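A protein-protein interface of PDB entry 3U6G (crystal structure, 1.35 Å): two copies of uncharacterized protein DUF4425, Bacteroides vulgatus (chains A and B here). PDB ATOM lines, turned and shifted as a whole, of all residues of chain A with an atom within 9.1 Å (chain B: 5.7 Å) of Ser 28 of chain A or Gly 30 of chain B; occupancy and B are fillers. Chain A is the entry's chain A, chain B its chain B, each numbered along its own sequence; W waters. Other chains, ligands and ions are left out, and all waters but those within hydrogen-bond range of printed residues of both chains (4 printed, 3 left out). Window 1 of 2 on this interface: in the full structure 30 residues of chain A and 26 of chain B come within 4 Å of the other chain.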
ATOM      1  N   ILE A  12       6.091   3.254  -4.371  1.00  0.00           N
ATOM      2  CA  ILE A  12       6.956   3.759  -3.323  1.00  0.00           C
ATOM      3  C   ILE A  12       8.380   3.823  -3.843  1.00  0.00           C
ATOM      4  O   ILE A  12       8.881   2.875  -4.415  1.00  0.00           O
ATOM      5  CB  ILE A  12       6.929   2.822  -2.086  1.00  0.00           C
ATOM      6  CG1 ILE A  12       5.551   2.854  -1.425  1.00  0.00           C
ATOM      7  CG2 ILE A  12       8.046   3.164  -1.085  1.00  0.00           C
ATOM      8  CD1 ILE A  12       5.258   4.066  -0.590  1.00  0.00           C
ATOM      9  N   ILE A  14      12.264   4.728  -2.386  1.00  0.00           N
ATOM     10  CA  ILE A  14      13.091   4.965  -1.203  1.00  0.00           C
ATOM     11  C   ILE A  14      14.490   5.370  -1.634  1.00  0.00           C
ATOM     12  O   ILE A  14      15.090   4.732  -2.505  1.00  0.00           O
ATOM     13  CB  ILE A  14      13.181   3.707  -0.301  1.00  0.00           C
ATOM     14  CG1 ILE A  14      11.773   3.249   0.093  1.00  0.00           C
ATOM     15  CG2 ILE A  14      14.022   4.001   0.922  1.00  0.00           C
ATOM     16  CD1 ILE A  14      11.706   1.888   0.727  1.00  0.00           C
ATOM     17  N   VAL A  25      19.026  -0.577   7.105  1.00  0.00           N
ATOM     18  CA  VAL A  25      17.701  -0.080   6.765  1.00  0.00           C
ATOM     19  C   VAL A  25      16.931  -1.191   6.068  1.00  0.00           C
ATOM     20  O   VAL A  25      17.358  -1.688   5.024  1.00  0.00           O
ATOM     21  CB  VAL A  25      17.772   1.140   5.823  1.00  0.00           C
ATOM     22  CG1 VAL A  25      16.369   1.684   5.595  1.00  0.00           C
ATOM     23  CG2 VAL A  25      18.707   2.221   6.403  1.00  0.00           C
ATOM     24  N   SER A  26      15.821  -1.601   6.661  1.00  0.00           N
ATOM     25  CA  SER A  26      14.981  -2.660   6.117  1.00  0.00           C
ATOM     26  C   SER A  26      13.579  -2.123   5.895  1.00  0.00           C
ATOM     27  O   SER A  26      13.114  -1.307   6.683  1.00  0.00           O
ATOM     28  CB  SER A  26      14.941  -3.838   7.086  1.00  0.00           C
ATOM     29  OG  SER A  26      16.206  -4.464   7.151  1.00  0.00           O
ATOM     30  N   VAL A  27      12.912  -2.587   4.838  1.00  0.00           N
ATOM     31  CA  VAL A  27      11.536  -2.193   4.588  1.00  0.00           C
ATOM     32  C   VAL A  27      10.666  -3.400   4.248  1.00  0.00           C
ATOM     33  O   VAL A  27      11.153  -4.397   3.724  1.00  0.00           O
ATOM     34  CB  VAL A  27      11.401  -1.127   3.468  1.00  0.00           C
ATOM     35  CG1 VAL A  27      12.165   0.151   3.836  1.00  0.00           C
ATOM     36  CG2 VAL A  27      11.814  -1.696   2.093  1.00  0.00           C
ATOM     37  N   SER A  28       9.394  -3.254   4.596  1.00  0.00           N
ATOM     38  CA  SER A  28       8.348  -4.181   4.192  1.00  0.00           C
ATOM     39  C   SER A  28       7.294  -3.381   3.444  1.00  0.00           C
ATOM     40  O   SER A  28       6.866  -2.318   3.889  1.00  0.00           O
ATOM     41  CB  SER A  28       7.743  -4.889   5.395  1.00  0.00           C
ATOM     42  OG  SER A  28       8.617  -5.912   5.847  1.00  0.00           O
ATOM     43  N   ILE A  29       6.927  -3.876   2.262  1.00  0.00           N
ATOM     44  CA  ILE A  29       6.023  -3.175   1.366  1.00  0.00           C
ATOM     45  C   ILE A  29       4.881  -4.109   0.980  1.00  0.00           C
ATOM     46  O   ILE A  29       5.088  -5.301   0.769  1.00  0.00           O
ATOM     47  CB  ILE A  29       6.773  -2.693   0.104  1.00  0.00           C
ATOM     48  CG1 ILE A  29       7.784  -1.616   0.498  1.00  0.00           C
ATOM     49  CG2 ILE A  29       5.783  -2.199  -0.982  1.00  0.00           C
ATOM     50  CD1 ILE A  29       8.836  -1.344  -0.550  1.00  0.00           C
ATOM     51  N   GLY A  30       3.670  -3.575   0.990  1.00  0.00           N
ATOM     52  CA  GLY A  30       2.526  -4.309   0.521  1.00  0.00           C
ATOM     53  C   GLY A  30       1.439  -3.365   0.085  1.00  0.00           C
ATOM     54  O   GLY A  30       1.494  -2.167   0.320  1.00  0.00           O
ATOM     55  N   GLY A  31       0.415  -3.905  -0.540  1.00  0.00           N
ATOM     56  CA  GLY A  31      -0.749  -3.110  -0.900  1.00  0.00           C
ATOM     57  C   GLY A  31      -1.971  -3.986  -0.994  1.00  0.00           C
ATOM     58  O   GLY A  31      -1.922  -5.182  -0.669  1.00  0.00           O
ATOM     59  N   LEU A  40       3.092  -6.860  -6.797  1.00  0.00           N
ATOM     60  CA  LEU A  40       4.166  -5.890  -6.678  1.00  0.00           C
ATOM     61  C   LEU A  40       5.232  -6.136  -7.755  1.00  0.00           C
ATOM     62  O   LEU A  40       5.509  -7.275  -8.108  1.00  0.00           O
ATOM     63  CB  LEU A  40       4.825  -6.001  -5.291  1.00  0.00           C
ATOM     64  CG  LEU A  40       3.893  -5.850  -4.085  1.00  0.00           C
ATOM     65  CD1 LEU A  40       4.645  -6.190  -2.785  1.00  0.00           C
ATOM     66  CD2 LEU A  40       3.240  -4.481  -4.012  1.00  0.00           C
ATOM     67  N   SER A  51       4.033  -9.827  -1.669  1.00  0.00           N
ATOM     68  CA  SER A  51       4.627  -9.242  -0.470  1.00  0.00           C
ATOM     69  C   SER A  51       6.072  -8.977  -0.824  1.00  0.00           C
ATOM     70  O   SER A  51       6.623  -9.598  -1.720  1.00  0.00           O
ATOM     71  CB  SER A  51       4.544 -10.189   0.736  1.00  0.00           C
ATOM     72  OG  SER A  51       5.335 -11.350   0.552  1.00  0.00           O
ATOM     73  N   TYR A  52       6.701  -8.072  -0.093  1.00  0.00           N
ATOM     74  CA  TYR A  52       8.088  -7.712  -0.370  1.00  0.00           C
ATOM     75  C   TYR A  52       8.749  -7.104   0.851  1.00  0.00           C
ATOM     76  O   TYR A  52       8.164  -6.262   1.526  1.00  0.00           O
ATOM     77  CB  TYR A  52       8.130  -6.731  -1.536  1.00  0.00           C
ATOM     78  CG  TYR A  52       9.505  -6.357  -2.019  1.00  0.00           C
ATOM     79  CD1 TYR A  52      10.456  -7.321  -2.322  1.00  0.00           C
ATOM     80  CD2 TYR A  52       9.840  -5.027  -2.214  1.00  0.00           C
ATOM     81  CE1 TYR A  52      11.718  -6.963  -2.773  1.00  0.00           C
ATOM     82  CE2 TYR A  52      11.089  -4.667  -2.666  1.00  0.00           C
ATOM     83  CZ  TYR A  52      12.018  -5.632  -2.931  1.00  0.00           C
ATOM     84  OH  TYR A  52      13.254  -5.251  -3.382  1.00  0.00           O
ATOM     85  N   SER A  53       9.935  -7.609   1.165  1.00  0.00           N
ATOM     86  CA  SER A  53      10.812  -6.983   2.144  1.00  0.00           C
ATOM     87  C   SER A  53      12.211  -6.967   1.576  1.00  0.00           C
ATOM     88  O   SER A  53      12.591  -7.851   0.798  1.00  0.00           O
ATOM     89  CB  SER A  53      10.825  -7.765   3.450  1.00  0.00           C
ATOM     90  OG  SER A  53      11.407  -9.045   3.240  1.00  0.00           O
ATOM     91  N   ALA A  54      12.990  -5.972   1.969  1.00  0.00           N
ATOM     92  CA  ALA A  54      14.349  -5.871   1.486  1.00  0.00           C
ATOM     93  C   ALA A  54      15.154  -5.022   2.443  1.00  0.00           C
ATOM     94  O   ALA A  54      14.631  -4.111   3.057  1.00  0.00           O
ATOM     95  CB  ALA A  54      14.371  -5.245   0.067  1.00  0.00           C
ATOM     96  N   GLN A  55      16.425  -5.360   2.594  1.00  0.00           N
ATOM     97  CA  GLN A  55      17.359  -4.423   3.167  1.00  0.00           C
ATOM     98  C   GLN A  55      17.765  -3.451   2.045  1.00  0.00           C
ATOM     99  O   GLN A  55      18.052  -3.861   0.920  1.00  0.00           O
ATOM    100  CB  GLN A  55      18.566  -5.138   3.750  1.00  0.00           C
ATOM    101  CG  GLN A  55      19.452  -4.177   4.525  1.00  0.00           C
ATOM    102  CD  GLN A  55      20.782  -4.759   4.894  1.00  0.00           C
ATOM    103  OE1 GLN A  55      21.097  -4.894   6.078  1.00  0.00           O
ATOM    104  NE2 GLN A  55      21.586  -5.107   3.885  1.00  0.00           N
ATOM    105  N   ILE A  56      17.790  -2.159   2.353  1.00  0.00           N
ATOM    106  CA  ILE A  56      18.116  -1.136   1.359  1.00  0.00           C
ATOM    107  C   ILE A  56      19.643  -1.063   1.290  1.00  0.00           C
ATOM    108  O   ILE A  56      20.295  -0.751   2.279  1.00  0.00           O
ATOM    109  CB  ILE A  56      17.546   0.249   1.760  1.00  0.00           C
ATOM    110  CG1 ILE A  56      16.030   0.185   2.004  1.00  0.00           C
ATOM    111  CG2 ILE A  56      17.861   1.292   0.697  1.00  0.00           C
ATOM    112  CD1 ILE A  56      15.239  -0.267   0.823  1.00  0.00           C
ATOM    113  N   MET A  61      15.629   2.565  -4.440  1.00  0.00           N
ATOM    114  CA  MET A  61      14.783   1.392  -4.672  1.00  0.00           C
ATOM    115  C   MET A  61      13.367   1.870  -4.952  1.00  0.00           C
ATOM    116  O   MET A  61      12.912   2.818  -4.332  1.00  0.00           O
ATOM    117  CB  MET A  61      14.764   0.501  -3.424  1.00  0.00           C
ATOM    118  CG  MET A  61      13.462  -0.296  -3.227  1.00  0.00           C
ATOM    119  SD  MET A  61      13.594  -1.674  -1.898  1.00  0.00           S
ATOM    120  CE  MET A  61      15.115  -2.650  -2.650  1.00  0.00           C
ATOM    121  N   CYS A  63       9.180   0.313  -5.860  1.00  0.00           N
ATOM    122  CA  CYS A  63       8.248  -0.794  -5.923  1.00  0.00           C
ATOM    123  C   CYS A  63       6.898  -0.216  -6.345  1.00  0.00           C
ATOM    124  O   CYS A  63       6.499   0.824  -5.848  1.00  0.00           O
ATOM    125  CB  CYS A  63       8.153  -1.480  -4.529  1.00  0.00           C
ATOM    126  SG  CYS A  63       7.095  -2.953  -4.521  1.00  0.00           S
ATOM    127  N   MET A  72      -1.168   1.238  -0.861  1.00  0.00           N
ATOM    128  CA  MET A  72       0.167   0.680  -0.767  1.00  0.00           C
ATOM    129  C   MET A  72       0.830   1.296   0.460  1.00  0.00           C
ATOM    130  O   MET A  72       0.601   2.458   0.769  1.00  0.00           O
ATOM    131  CB  MET A  72       0.991   0.948  -2.041  1.00  0.00           C
ATOM    132  CG  MET A  72       2.312   0.049  -2.291  1.00  0.00           C
ATOM    133  SD  MET A  72       3.215   0.742  -3.723  1.00  0.00           S
ATOM    134  CE  MET A  72       4.282  -0.821  -4.057  1.00  0.00           C
ATOM    135  N   THR A  73       1.609   0.485   1.160  1.00  0.00           N
ATOM    136  CA  THR A  73       2.279   0.858   2.415  1.00  0.00           C
ATOM    137  C   THR A  73       3.730   0.438   2.415  1.00  0.00           C
ATOM    138  O   THR A  73       4.068  -0.592   1.825  1.00  0.00           O
ATOM    139  CB  THR A  73       1.668   0.100   3.608  1.00  0.00           C
ATOM    140  OG1 THR A  73       1.707  -1.322   3.366  1.00  0.00           O
ATOM    141  CG2 THR A  73       0.252   0.533   3.832  1.00  0.00           C
ATOM    142  N   CYS A  74       4.573   1.200   3.105  1.00  0.00           N
ATOM    143  CA  CYS A  74       5.962   0.863   3.314  1.00  0.00           C
ATOM    144  C   CYS A  74       6.260   1.137   4.776  1.00  0.00           C
ATOM    145  O   CYS A  74       6.069   2.270   5.248  1.00  0.00           O
ATOM    146  CB  CYS A  74       6.862   1.729   2.423  1.00  0.00           C
ATOM    147  SG  CYS A  74       8.641   1.489   2.696  1.00  0.00           S
ATOM    148  N   ALA A  75       6.680   0.091   5.479  1.00  0.00           N
ATOM    149  CA  ALA A  75       7.138   0.186   6.869  1.00  0.00           C
ATOM    150  C   ALA A  75       8.607  -0.137   6.927  1.00  0.00           C
ATOM    151  O   ALA A  75       9.073  -1.090   6.322  1.00  0.00           O
ATOM    152  CB  ALA A  75       6.352  -0.770   7.781  1.00  0.00           C
ATOM    153  N   GLY A  76       9.359   0.663   7.662  1.00  0.00           N
ATOM    154  CA  GLY A  76      10.787   0.471   7.715  1.00  0.00           C
ATOM    155  C   GLY A  76      11.387   0.557   9.099  1.00  0.00           C
ATOM    156  O   GLY A  76      10.803   1.113  10.020  1.00  0.00           O
ATOM    157  N   SER A  77      12.575  -0.025   9.207  1.00  0.00           N
ATOM    158  CA  SER A  77      13.371   0.142  10.412  1.00  0.00           C
ATOM    159  C   SER A  77      14.767   0.563  10.037  1.00  0.00           C
ATOM    160  O   SER A  77      15.314   0.184   8.996  1.00  0.00           O
ATOM    161  CB  SER A  77      13.431  -1.131  11.256  1.00  0.00           C
ATOM    162  OG  SER A  77      14.184  -2.118  10.594  1.00  0.00           O
ATOM    163  N   VAL A  92      11.249   8.649   1.666  1.00  0.00           N
ATOM    164  CA  VAL A  92      10.297   7.680   1.127  1.00  0.00           C
ATOM    165  C   VAL A  92       9.128   8.452   0.526  1.00  0.00           C
ATOM    166  O   VAL A  92       8.504   9.262   1.211  1.00  0.00           O
ATOM    167  CB  VAL A  92       9.780   6.718   2.205  1.00  0.00           C
ATOM    168  CG1 VAL A  92       8.879   5.663   1.566  1.00  0.00           C
ATOM    169  CG2 VAL A  92      10.938   6.057   2.947  1.00  0.00           C
ATOM    170  N   PHE A 119       9.580   3.737  10.729  1.00  0.00           N
ATOM    171  CA  PHE A 119       8.796   4.685   9.978  1.00  0.00           C
ATOM    172  C   PHE A 119       7.761   3.961   9.163  1.00  0.00           C
ATOM    173  O   PHE A 119       7.880   2.744   8.918  1.00  0.00           O
ATOM    174  CB  PHE A 119       9.697   5.543   9.089  1.00  0.00           C
ATOM    175  CG  PHE A 119      10.482   4.767   8.045  1.00  0.00           C
ATOM    176  CD1 PHE A 119       9.877   4.337   6.869  1.00  0.00           C
ATOM    177  CD2 PHE A 119      11.842   4.517   8.221  1.00  0.00           C
ATOM    178  CE1 PHE A 119      10.607   3.634   5.906  1.00  0.00           C
ATOM    179  CE2 PHE A 119      12.574   3.824   7.267  1.00  0.00           C
ATOM    180  CZ  PHE A 119      11.957   3.379   6.105  1.00  0.00           C
ATOM    181  N   SER A 120       6.751   4.711   8.742  1.00  0.00           N
ATOM    182  CA  SER A 120       5.720   4.170   7.875  1.00  0.00           C
ATOM    183  C   SER A 120       5.185   5.264   6.981  1.00  0.00           C
ATOM    184  O   SER A 120       5.034   6.401   7.412  1.00  0.00           O
ATOM    185  CB  SER A 120       4.568   3.567   8.696  1.00  0.00           C
ATOM    186  OG  SER A 120       3.638   2.879   7.872  1.00  0.00           O
ATOM    187  N   VAL A 121       4.919   4.910   5.734  1.00  0.00           N
ATOM    188  CA  VAL A 121       4.215   5.801   4.824  1.00  0.00           C
ATOM    189  C   VAL A 121       3.317   4.992   3.916  1.00  0.00           C
ATOM    190  O   VAL A 121       3.616   3.848   3.581  1.00  0.00           O
ATOM    191  CB  VAL A 121       5.186   6.683   4.010  1.00  0.00           C
ATOM    192  CG1 VAL A 121       6.000   5.871   3.069  1.00  0.00           C
ATOM    193  CG2 VAL A 121       4.423   7.808   3.276  1.00  0.00           C
ATOM    194  N   SER B  28      -0.450  -7.412   5.267  1.00  0.00           N
ATOM    195  CA  SER B  28       0.953  -7.538   4.917  1.00  0.00           C
ATOM    196  C   SER B  28       1.724  -7.440   6.222  1.00  0.00           C
ATOM    197  O   SER B  28       1.438  -6.560   7.035  1.00  0.00           O
ATOM    198  CB  SER B  28       1.356  -6.438   3.958  1.00  0.00           C
ATOM    199  OG  SER B  28       0.936  -6.734   2.628  1.00  0.00           O
ATOM    200  N   ILE B  29       2.664  -8.357   6.434  1.00  0.00           N
ATOM    201  CA  ILE B  29       3.420  -8.440   7.682  1.00  0.00           C
ATOM    202  C   ILE B  29       4.914  -8.524   7.376  1.00  0.00           C
ATOM    203  O   ILE B  29       5.338  -9.195   6.430  1.00  0.00           O
ATOM    204  CB  ILE B  29       2.965  -9.658   8.503  1.00  0.00           C
ATOM    205  CG1 ILE B  29       1.488  -9.491   8.893  1.00  0.00           C
ATOM    206  CG2 ILE B  29       3.830  -9.832   9.778  1.00  0.00           C
ATOM    207  CD1 ILE B  29       0.916 -10.668   9.660  1.00  0.00           C
ATOM    208  N   GLY B  30       5.706  -7.819   8.170  1.00  0.00           N
ATOM    209  CA  GLY B  30       7.141  -7.932   8.091  1.00  0.00           C
ATOM    210  C   GLY B  30       7.763  -7.499   9.410  1.00  0.00           C
ATOM    211  O   GLY B  30       7.106  -6.889  10.264  1.00  0.00           O
ATOM    212  N   GLY B  31       9.030  -7.832   9.586  1.00  0.00           N
ATOM    213  CA  GLY B  31       9.761  -7.412  10.770  1.00  0.00           C
ATOM    214  C   GLY B  31      11.211  -7.211  10.449  1.00  0.00           C
ATOM    215  O   GLY B  31      11.622  -7.316   9.281  1.00  0.00           O
ATOM    216  N   ALA B  32      11.994  -6.900  11.482  1.00  0.00           N
ATOM    217  CA  ALA B  32      13.403  -6.610  11.276  1.00  0.00           C
ATOM    218  C   ALA B  32      14.237  -7.108  12.436  1.00  0.00           C
ATOM    219  O   ALA B  32      13.783  -7.153  13.595  1.00  0.00           O
ATOM    220  CB  ALA B  32      13.645  -5.107  11.062  1.00  0.00           C
ATOM    221  N   PRO B  37      15.440  -7.856   7.041  1.00  0.00           N
ATOM    222  CA  PRO B  37      14.103  -8.375   7.304  1.00  0.00           C
ATOM    223  C   PRO B  37      14.135  -9.667   8.118  1.00  0.00           C
ATOM    224  O   PRO B  37      14.962 -10.540   7.867  1.00  0.00           O
ATOM    225  CB  PRO B  37      13.547  -8.613   5.907  1.00  0.00           C
ATOM    226  CG  PRO B  37      14.258  -7.636   5.054  1.00  0.00           C
ATOM    227  CD  PRO B  37      15.648  -7.574   5.617  1.00  0.00           C
ATOM    228  N   LEU B  40       9.932 -15.022   9.156  1.00  0.00           N
ATOM    229  CA  LEU B  40       8.588 -15.111   9.701  1.00  0.00           C
ATOM    230  C   LEU B  40       8.118 -16.541   9.747  1.00  0.00           C
ATOM    231  O   LEU B  40       8.466 -17.335   8.871  1.00  0.00           O
ATOM    232  CB  LEU B  40       7.616 -14.284   8.856  1.00  0.00           C
ATOM    233  CG  LEU B  40       7.992 -12.817   8.640  1.00  0.00           C
ATOM    234  CD1 LEU B  40       7.040 -12.239   7.607  1.00  0.00           C
ATOM    235  CD2 LEU B  40       7.979 -12.024   9.952  1.00  0.00           C
ATOM    236  N   ASP B  50      10.395 -14.050   4.528  1.00  0.00           N
ATOM    237  CA  ASP B  50      10.717 -12.825   5.272  1.00  0.00           C
ATOM    238  C   ASP B  50       9.860 -11.634   4.845  1.00  0.00           C
ATOM    239  O   ASP B  50      10.153 -10.489   5.175  1.00  0.00           O
ATOM    240  CB  ASP B  50      12.208 -12.504   5.289  1.00  0.00           C
ATOM    241  CG  ASP B  50      12.788 -12.262   3.939  1.00  0.00           C
ATOM    242  OD1 ASP B  50      12.049 -11.959   2.983  1.00  0.00           O
ATOM    243  OD2 ASP B  50      14.047 -12.330   3.839  1.00  0.00           O
ATOM    244  N   SER B  51       8.775 -11.948   4.156  1.00  0.00           N
ATOM    245  CA  SER B  51       7.655 -11.061   3.936  1.00  0.00           C
ATOM    246  C   SER B  51       6.450 -11.964   3.837  1.00  0.00           C
ATOM    247  O   SER B  51       6.557 -13.114   3.460  1.00  0.00           O
ATOM    248  CB  SER B  51       7.827 -10.242   2.658  1.00  0.00           C
ATOM    249  OG  SER B  51       7.908 -11.072   1.514  1.00  0.00           O
ATOM    250  N   TYR B  52       5.288 -11.445   4.172  1.00  0.00           N
ATOM    251  CA  TYR B  52       4.087 -12.234   4.135  1.00  0.00           C
ATOM    252  C   TYR B  52       2.878 -11.368   3.879  1.00  0.00           C
ATOM    253  O   TYR B  52       2.748 -10.290   4.462  1.00  0.00           O
ATOM    254  CB  TYR B  52       3.907 -12.970   5.456  1.00  0.00           C
ATOM    255  CG  TYR B  52       2.727 -13.920   5.460  1.00  0.00           C
ATOM    256  CD1 TYR B  52       2.773 -15.129   4.757  1.00  0.00           C
ATOM    257  CD2 TYR B  52       1.575 -13.618   6.162  1.00  0.00           C
ATOM    258  CE1 TYR B  52       1.698 -16.010   4.762  1.00  0.00           C
ATOM    259  CE2 TYR B  52       0.480 -14.500   6.177  1.00  0.00           C
ATOM    260  CZ  TYR B  52       0.556 -15.685   5.482  1.00  0.00           C
ATOM    261  OH  TYR B  52      -0.510 -16.550   5.496  1.00  0.00           O
ATOM    262  N   PHE B  71      11.583  -5.548  15.749  1.00  0.00           N
ATOM    263  CA  PHE B  71      10.465  -4.829  15.159  1.00  0.00           C
ATOM    264  C   PHE B  71       9.590  -5.774  14.373  1.00  0.00           C
ATOM    265  O   PHE B  71      10.097  -6.659  13.701  1.00  0.00           O
ATOM    266  CB  PHE B  71      11.009  -3.738  14.229  1.00  0.00           C
ATOM    267  CG  PHE B  71       9.976  -3.005  13.411  1.00  0.00           C
ATOM    268  CD1 PHE B  71       9.004  -2.226  14.019  1.00  0.00           C
ATOM    269  CD2 PHE B  71      10.028  -3.051  12.022  1.00  0.00           C
ATOM    270  CE1 PHE B  71       8.081  -1.513  13.262  1.00  0.00           C
ATOM    271  CE2 PHE B  71       9.128  -2.340  11.251  1.00  0.00           C
ATOM    272  CZ  PHE B  71       8.143  -1.581  11.869  1.00  0.00           C
ATOM    273  N   MET B  72       8.278  -5.597  14.482  1.00  0.00           N
ATOM    274  CA  MET B  72       7.341  -6.261  13.592  1.00  0.00           C
ATOM    275  C   MET B  72       6.216  -5.296  13.274  1.00  0.00           C
ATOM    276  O   MET B  72       5.881  -4.458  14.097  1.00  0.00           O
ATOM    277  CB  MET B  72       6.791  -7.518  14.262  1.00  0.00           C
ATOM    278  CG  MET B  72       6.285  -8.564  13.310  1.00  0.00           C
ATOM    279  SD  MET B  72       5.854 -10.209  14.214  1.00  0.00           S
ATOM    280  CE  MET B  72       5.505 -11.257  12.614  1.00  0.00           C
ATOM    281  N   THR B  73       5.635  -5.429  12.091  1.00  0.00           N
ATOM    282  CA  THR B  73       4.531  -4.608  11.721  1.00  0.00           C
ATOM    283  C   THR B  73       3.532  -5.364  10.838  1.00  0.00           C
ATOM    284  O   THR B  73       3.891  -6.280  10.105  1.00  0.00           O
ATOM    285  CB  THR B  73       5.018  -3.324  11.055  1.00  0.00           C
ATOM    286  OG1 THR B  73       3.942  -2.383  10.998  1.00  0.00           O
ATOM    287  CG2 THR B  73       5.553  -3.611   9.677  1.00  0.00           C
ATOM    288  N   CYS B  74       2.275  -4.952  10.956  1.00  0.00           N
ATOM    289  CA  CYS B  74       1.161  -5.507  10.208  1.00  0.00           C
ATOM    290  C   CYS B  74       0.355  -4.349   9.646  1.00  0.00           C
ATOM    291  O   CYS B  74      -0.080  -3.484  10.418  1.00  0.00           O
ATOM    292  CB  CYS B  74       0.279  -6.335  11.145  1.00  0.00           C
ATOM    293  SG  CYS B  74      -1.242  -6.970  10.405  1.00  0.00           S
HETATM  294  O   HOH W   1      -1.695  -6.204   1.573  1.00  0.00           O
HETATM  295  O   HOH W   2      10.921  -5.896   7.027  1.00  0.00           O
HETATM  296  O   HOH W   3       7.476 -13.813   0.757  1.00  0.00           O
HETATM  297  O   HOH W   4       6.669  -7.809   4.418  1.00  0.00           O
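The backbone carbonyl oxygen of Asp 50 of chain B lies within hydrogen-bond range of the side-chain hydroxyl of Ser 53 of chain A (2.7 Å).
OG of Ser 26 of chain A lies close to N of Pro 37 of chain B (3.5 Å).
OG of Ser 51 of chain A lies within hydrogen-bond range of OG of Ser 51 of chain B.
The backbone NH of Ala 32 of chain B lies within hydrogen-bond range of the backbone carbonyl oxygen of Phe 71 of chain B (2.9 Å).
The backbone carbonyl oxygen (O) of Gly 30 of chain B sits at hydrogen-bond distance from the backbone NH (N) of Thr 73 of chain B.
O of Gly 30 of chain A lies within hydrogen-bond range of N of Thr 73 of chain A.
N of Ile 29 of chain B sits at hydrogen-bond distance from O of Tyr 52 of chain B.
N of Ile 29 of chain A sits at hydrogen-bond distance from O of Tyr 52 of chain A, at 2.8 Å.
The backbone NH (N) of Val 27 of chain A is in hydrogen-bond range of the backbone carbonyl oxygen (O) of Ala 54 of chain A.
Among the printed residues, merely in contact across the chains: Ser 77 of chain A with Ala 32 of chain B (3.1 Å), Ser 28 of chain A with Gly 30 of chain B (3.4 Å), Ser 53 of chain A with Pro 37 of chain B (3.4 Å), Ala 75 of chain A with Thr 73 of chain B (3.5 Å), Gly 30 of chain A with Ser 28 of chain B (3.6 Å), Tyr 52 of chain A with Ser 51 of chain B (3.6 Å), Ser 51 of chain A with Tyr 52 of chain B (3.6 Å), Ser 53 of chain A with Ser 51 of chain B (3.7 Å), Ala 54 of chain A with Pro 37 of chain B (3.7 Å), Gln 55 of chain A with Pro 37 of chain B (3.8 Å) and Ser 77 of chain A with Phe 71 of chain B (3.98 Å).
Printed residues of chain B within 4 Å of Ser 28 of chain A: Gly 30 (3.4 Å).
Ile 29 of chain A touches none of the printed residues of chain B.
Printed residues of chain B within 4 Å of Gly 30 of chain A: Ser 28 (3.6 Å).
Printed residues of chain B within 4 Å of Ser 77 of chain A: Ala 32 (3.1 Å) and Phe 71 (3.98 Å).
No residue of chain A comes within 4 Å of Gly 31 of chain B.
Of the printed residues of chain A, Phe 71 of chain B touches Ser 77.
The nearest printed residue of chain B that does not touch Tyr 52 of chain A is Tyr 52 of chain B (5.6 Å).
Of the 14 printed residues of chain B, 9 touch a printed residue of chain A.
Printed residues of chain B that touch a printed residue of chain A: Ser 28, Gly 30, Ala 32, Pro 37, Asp 50, Ser 51, Tyr 52, Phe 71 and Thr 73.
Of the 28 printed residues of chain A, 10 touch a printed residue of chain B.
Hydrophobic or aromatic side chains of chain A that line the printed part of chain B: Ala 75.
Among the printed residues, 14 pairs touch across the chains.
Ser 28 of chain A touches Gly 30 of chain B, and with the chains exchanged Gly 30 of chain A touches Ser 28 of chain B.
Ser 51 of chain A touches its own counterpart, Ser 51 of chain B.
Ser 51 of chain A touches Tyr 52 of chain B, and with the chains exchanged Tyr 52 of chain A touches Ser 51 of chain B.
Of the 14 pairs that touch across the chains among the printed residues, 5 have their exchanged pair printed and touching as well.
Water W1 lies within hydrogen-bond range of O of Gly 31 of chain A and OG of Ser 28 of chain B.
Water W2 bridges OG of Ser 28 of chain A (2.6 Å) and O of Gly 31 of chain B (2.8 Å).
Water W4 bridges the backbone carbonyl oxygen of Ile 29 of chain B and the side-chain hydroxyl of Ser 28 of chain A.
Water W3 bridges OG of Ser 51 of chain B (2.9 Å) and OG of Ser 51 of chain A (3.3 Å).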
